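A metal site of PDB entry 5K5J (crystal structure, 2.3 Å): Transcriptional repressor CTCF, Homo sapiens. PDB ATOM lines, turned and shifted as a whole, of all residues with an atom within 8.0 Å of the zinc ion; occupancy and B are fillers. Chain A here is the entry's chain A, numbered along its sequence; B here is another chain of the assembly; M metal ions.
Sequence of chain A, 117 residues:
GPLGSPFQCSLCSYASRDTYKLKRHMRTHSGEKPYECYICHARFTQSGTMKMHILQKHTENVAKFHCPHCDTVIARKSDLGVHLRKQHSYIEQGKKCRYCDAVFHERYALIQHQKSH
A ring nitrogen (ND1) of His 83 is in hydrogen-bond range of OP1 of DG 3 of chain B (2.6 Å). The side-chain hydroxyl of Thr 72 lies close to the side-chain sulfur of Cys 70, at 3.4 Å. The backbone NH (N) of His 69 sits close to the side-chain sulfur (SG) of Cys 67. The backbone carbonyl oxygen (O) of Thr 72 is in hydrogen-bond range of the backbone NH (N) of Cys 67, 3.0 Å away.
The zinc ion is bound by a ring nitrogen (NE2) of His 88 (2.0 Å), a ring nitrogen (NE2) of His 83 (2.0 Å), the side-chain sulfur (SG) of Cys 70 (2.2 Å) and the side-chain sulfur (SG) of Cys 67 (2.3 Å).
Four residues have an atom within 4 Å of the zinc ion: Cys 67, Cys 70, His 83 and His 88.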
ATOM      1  N   HIS A  66       4.642 -26.805  -2.742  1.00  0.00           N
ATOM      2  CA  HIS A  66       3.618 -27.276  -1.822  1.00  0.00           C
ATOM      3  C   HIS A  66       4.179 -28.398  -0.956  1.00  0.00           C
ATOM      4  O   HIS A  66       4.823 -29.318  -1.461  1.00  0.00           O
ATOM      5  CB  HIS A  66       2.391 -27.773  -2.577  1.00  0.00           C
ATOM      6  CG  HIS A  66       1.701 -26.715  -3.385  1.00  0.00           C
ATOM      7  ND1 HIS A  66       0.419 -26.300  -3.117  1.00  0.00           N
ATOM      8  CD2 HIS A  66       2.125 -26.010  -4.457  1.00  0.00           C
ATOM      9  CE1 HIS A  66       0.073 -25.364  -3.997  1.00  0.00           C
ATOM     10  NE2 HIS A  66       1.090 -25.174  -4.809  1.00  0.00           N
ATOM     11  N   CYS A  67       3.931 -28.315   0.352  1.00  0.00           N
ATOM     12  CA  CYS A  67       4.316 -29.400   1.240  1.00  0.00           C
ATOM     13  C   CYS A  67       3.489 -30.636   0.919  1.00  0.00           C
ATOM     14  O   CYS A  67       2.272 -30.531   0.756  1.00  0.00           O
ATOM     15  CB  CYS A  67       4.131 -28.998   2.697  1.00  0.00           C
ATOM     16  SG  CYS A  67       4.604 -30.273   3.890  1.00  0.00           S
ATOM     17  N   PRO A  68       4.111 -31.819   0.808  1.00  0.00           N
ATOM     18  CA  PRO A  68       3.320 -33.035   0.530  1.00  0.00           C
ATOM     19  C   PRO A  68       2.513 -33.523   1.719  1.00  0.00           C
ATOM     20  O   PRO A  68       1.706 -34.443   1.541  1.00  0.00           O
ATOM     21  CB  PRO A  68       4.389 -34.053   0.125  1.00  0.00           C
ATOM     22  CG  PRO A  68       5.640 -33.570   0.796  1.00  0.00           C
ATOM     23  CD  PRO A  68       5.555 -32.071   0.801  1.00  0.00           C
ATOM     24  N   HIS A  69       2.684 -32.945   2.912  1.00  0.00           N
ATOM     25  CA  HIS A  69       1.983 -33.419   4.101  1.00  0.00           C
ATOM     26  C   HIS A  69       0.991 -32.414   4.670  1.00  0.00           C
ATOM     27  O   HIS A  69       0.199 -32.777   5.549  1.00  0.00           O
ATOM     28  CB  HIS A  69       2.996 -33.799   5.183  1.00  0.00           C
ATOM     29  CG  HIS A  69       3.984 -34.853   4.753  1.00  0.00           C
ATOM     30  ND1 HIS A  69       5.294 -34.551   4.421  1.00  0.00           N
ATOM     31  CD2 HIS A  69       3.840 -36.184   4.573  1.00  0.00           C
ATOM     32  CE1 HIS A  69       5.915 -35.666   4.070  1.00  0.00           C
ATOM     33  NE2 HIS A  69       5.057 -36.668   4.155  1.00  0.00           N
ATOM     34  N   CYS A  70       1.008 -31.167   4.200  1.00  0.00           N
ATOM     35  CA  CYS A  70       0.006 -30.180   4.604  1.00  0.00           C
ATOM     36  C   CYS A  70      -0.188 -29.195   3.458  1.00  0.00           C
ATOM     37  O   CYS A  70       0.461 -29.293   2.413  1.00  0.00           O
ATOM     38  CB  CYS A  70       0.421 -29.472   5.904  1.00  0.00           C
ATOM     39  SG  CYS A  70       1.825 -28.354   5.755  1.00  0.00           S
ATOM     40  N   ASP A  71      -1.089 -28.239   3.663  1.00  0.00           N
ATOM     41  CA  ASP A  71      -1.442 -27.277   2.623  1.00  0.00           C
ATOM     42  C   ASP A  71      -0.526 -26.066   2.586  1.00  0.00           C
ATOM     43  O   ASP A  71      -0.783 -25.135   1.814  1.00  0.00           O
ATOM     44  CB  ASP A  71      -2.897 -26.824   2.813  1.00  0.00           C
ATOM     45  CG  ASP A  71      -3.220 -26.474   4.258  1.00  0.00           C
ATOM     46  OD1 ASP A  71      -2.316 -26.018   4.988  1.00  0.00           O
ATOM     47  OD2 ASP A  71      -4.389 -26.652   4.662  1.00  0.00           O
ATOM     48  N   THR A  72       0.544 -26.044   3.389  1.00  0.00           N
ATOM     49  CA  THR A  72       1.446 -24.902   3.396  1.00  0.00           C
ATOM     50  C   THR A  72       2.201 -24.799   2.081  1.00  0.00           C
ATOM     51  O   THR A  72       2.742 -25.793   1.588  1.00  0.00           O
ATOM     52  CB  THR A  72       2.430 -25.002   4.568  1.00  0.00           C
ATOM     53  OG1 THR A  72       1.697 -24.998   5.800  1.00  0.00           O
ATOM     54  CG2 THR A  72       3.411 -23.845   4.555  1.00  0.00           C
ATOM     55  N   VAL A  73       2.226 -23.601   1.501  1.00  0.00           N
ATOM     56  CA  VAL A  73       2.967 -23.319   0.270  1.00  0.00           C
ATOM     57  C   VAL A  73       4.142 -22.428   0.634  1.00  0.00           C
ATOM     58  O   VAL A  73       3.989 -21.447   1.372  1.00  0.00           O
ATOM     59  CB  VAL A  73       2.065 -22.656  -0.774  1.00  0.00           C
ATOM     60  CG1 VAL A  73       2.851 -22.356  -2.039  1.00  0.00           C
ATOM     61  CG2 VAL A  73       0.877 -23.547  -1.085  1.00  0.00           C
ATOM     62  N   ILE A  74       5.331 -22.778   0.122  1.00  0.00           N
ATOM     63  CA  ILE A  74       6.578 -22.136   0.512  1.00  0.00           C
ATOM     64  C   ILE A  74       7.341 -21.732  -0.739  1.00  0.00           C
ATOM     65  O   ILE A  74       7.381 -22.477  -1.729  1.00  0.00           O
ATOM     66  CB  ILE A  74       7.419 -23.049   1.417  1.00  0.00           C
ATOM     67  CG1 ILE A  74       6.641 -23.379   2.688  1.00  0.00           C
ATOM     68  CG2 ILE A  74       8.743 -22.415   1.758  1.00  0.00           C
ATOM     69  CD1 ILE A  74       7.438 -24.140   3.714  1.00  0.00           C
ATOM     70  N   LEU A  80      11.187 -25.180   2.270  1.00  0.00           N
ATOM     71  CA  LEU A  80      10.332 -26.341   2.441  1.00  0.00           C
ATOM     72  C   LEU A  80      11.060 -27.443   3.196  1.00  0.00           C
ATOM     73  O   LEU A  80      10.465 -28.161   4.002  1.00  0.00           O
ATOM     74  CB  LEU A  80       9.837 -26.836   1.083  1.00  0.00           C
ATOM     75  CG  LEU A  80       9.024 -28.135   1.087  1.00  0.00           C
ATOM     76  CD1 LEU A  80       7.822 -28.030   2.032  1.00  0.00           C
ATOM     77  CD2 LEU A  80       8.589 -28.501  -0.328  1.00  0.00           C
ATOM     78  N   HIS A  83      10.785 -26.564   6.789  1.00  0.00           N
ATOM     79  CA  HIS A  83       9.430 -26.943   7.195  1.00  0.00           C
ATOM     80  C   HIS A  83       9.317 -28.446   7.391  1.00  0.00           C
ATOM     81  O   HIS A  83       8.782 -28.917   8.407  1.00  0.00           O
ATOM     82  CB  HIS A  83       8.434 -26.450   6.144  1.00  0.00           C
ATOM     83  CG  HIS A  83       7.032 -26.908   6.376  1.00  0.00           C
ATOM     84  ND1 HIS A  83       6.103 -26.155   7.064  1.00  0.00           N
ATOM     85  CD2 HIS A  83       6.382 -28.045   5.996  1.00  0.00           C
ATOM     86  CE1 HIS A  83       4.948 -26.802   7.101  1.00  0.00           C
ATOM     87  NE2 HIS A  83       5.101 -27.954   6.469  1.00  0.00           N
ATOM     88  N   LEU A  84       9.820 -29.225   6.424  1.00  0.00           N
ATOM     89  CA  LEU A  84       9.750 -30.683   6.520  1.00  0.00           C
ATOM     90  C   LEU A  84      10.500 -31.191   7.748  1.00  0.00           C
ATOM     91  O   LEU A  84      10.029 -32.086   8.446  1.00  0.00           O
ATOM     92  CB  LEU A  84      10.303 -31.331   5.253  1.00  0.00           C
ATOM     93  CG  LEU A  84       9.492 -31.189   3.968  1.00  0.00           C
ATOM     94  CD1 LEU A  84      10.292 -31.690   2.770  1.00  0.00           C
ATOM     95  CD2 LEU A  84       8.170 -31.931   4.095  1.00  0.00           C
ATOM     96  N   GLN A  87       8.339 -29.760  11.017  1.00  0.00           N
ATOM     97  CA  GLN A  87       6.938 -30.117  11.228  1.00  0.00           C
ATOM     98  C   GLN A  87       6.626 -31.574  10.972  1.00  0.00           C
ATOM     99  O   GLN A  87       5.709 -32.119  11.595  1.00  0.00           O
ATOM    100  CB  GLN A  87       6.034 -29.252  10.344  1.00  0.00           C
ATOM    101  CG  GLN A  87       6.379 -27.760  10.331  1.00  0.00           C
ATOM    102  CD  GLN A  87       6.123 -27.077  11.662  1.00  0.00           C
ATOM    103  OE1 GLN A  87       5.445 -27.628  12.530  1.00  0.00           O
ATOM    104  NE2 GLN A  87       6.656 -25.877  11.819  1.00  0.00           N
ATOM    105  N   HIS A  88       7.342 -32.230  10.072  1.00  0.00           N
ATOM    106  CA  HIS A  88       6.992 -33.570   9.612  1.00  0.00           C
ATOM    107  C   HIS A  88       8.129 -34.559   9.835  1.00  0.00           C
ATOM    108  O   HIS A  88       8.376 -35.444   9.012  1.00  0.00           O
ATOM    109  CB  HIS A  88       6.579 -33.556   8.141  1.00  0.00           C
ATOM    110  CG  HIS A  88       5.520 -32.535   7.837  1.00  0.00           C
ATOM    111  ND1 HIS A  88       4.202 -32.693   8.221  1.00  0.00           N
ATOM    112  CD2 HIS A  88       5.584 -31.365   7.166  1.00  0.00           C
ATOM    113  CE1 HIS A  88       3.501 -31.657   7.810  1.00  0.00           C
ATOM    114  NE2 HIS A  88       4.313 -30.826   7.171  1.00  0.00           N
ATOM    115  N   TYR A 108       3.581 -31.373  13.418  1.00  0.00           N
ATOM    116  CA  TYR A 108       2.345 -31.014  12.720  1.00  0.00           C
ATOM    117  C   TYR A 108       1.148 -31.721  13.339  1.00  0.00           C
ATOM    118  O   TYR A 108       0.087 -31.104  13.532  1.00  0.00           O
ATOM    119  CB  TYR A 108       2.464 -31.362  11.240  1.00  0.00           C
ATOM    120  CG  TYR A 108       1.203 -31.121  10.450  1.00  0.00           C
ATOM    121  CD1 TYR A 108       0.838 -29.834  10.067  1.00  0.00           C
ATOM    122  CD2 TYR A 108       0.382 -32.171  10.079  1.00  0.00           C
ATOM    123  CE1 TYR A 108      -0.323 -29.601   9.350  1.00  0.00           C
ATOM    124  CE2 TYR A 108      -0.777 -31.954   9.353  1.00  0.00           C
ATOM    125  CZ  TYR A 108      -1.124 -30.665   8.995  1.00  0.00           C
ATOM    126  OH  TYR A 108      -2.277 -30.444   8.276  1.00  0.00           O
ATOM    127  P    DG B   3       7.201 -22.619   7.816  1.00  0.00           P
ATOM    128  OP1  DG B   3       6.127 -23.636   7.731  1.00  0.00           O
ATOM    129  OP2  DG B   3       8.599 -23.057   8.033  1.00  0.00           O
ATOM    130  O5'  DG B   3       7.171 -21.703   6.505  1.00  0.00           O
ATOM    131  C5'  DG B   3       6.014 -20.925   6.201  1.00  0.00           C
ATOM    132  C4'  DG B   3       6.393 -19.516   5.779  1.00  0.00           C
ATOM    133  O4'  DG B   3       7.128 -18.861   6.842  1.00  0.00           O
ATOM    134  C3'  DG B   3       7.276 -19.421   4.539  1.00  0.00           C
ATOM    135  O3'  DG B   3       6.902 -18.287   3.787  1.00  0.00           O
ATOM    136  C2'  DG B   3       8.673 -19.277   5.130  1.00  0.00           C
ATOM    137  C1'  DG B   3       8.386 -18.446   6.376  1.00  0.00           C
ATOM    138  N9   DG B   3       9.358 -18.635   7.446  1.00  0.00           N
ATOM    139  C8   DG B   3       9.726 -19.827   8.021  1.00  0.00           C
ATOM    140  N7   DG B   3      10.601 -19.685   8.979  1.00  0.00           N
ATOM    141  C5   DG B   3      10.817 -18.323   9.053  1.00  0.00           C
ATOM    142  C6   DG B   3      11.675 -17.576   9.898  1.00  0.00           C
ATOM    143  O6   DG B   3      12.425 -17.993  10.789  1.00  0.00           O
ATOM    144  N1   DG B   3      11.599 -16.215   9.638  1.00  0.00           N
ATOM    145  C2   DG B   3      10.802 -15.637   8.669  1.00  0.00           C
ATOM    146  N2   DG B   3      10.868 -14.303   8.564  1.00  0.00           N
ATOM    147  N3   DG B   3       9.999 -16.327   7.876  1.00  0.00           N
ATOM    148  C4   DG B   3      10.061 -17.651   8.119  1.00  0.00           C
HETATM  149 ZN    ZN M   1       3.806 -29.400   5.851  1.00  0.00          ZN
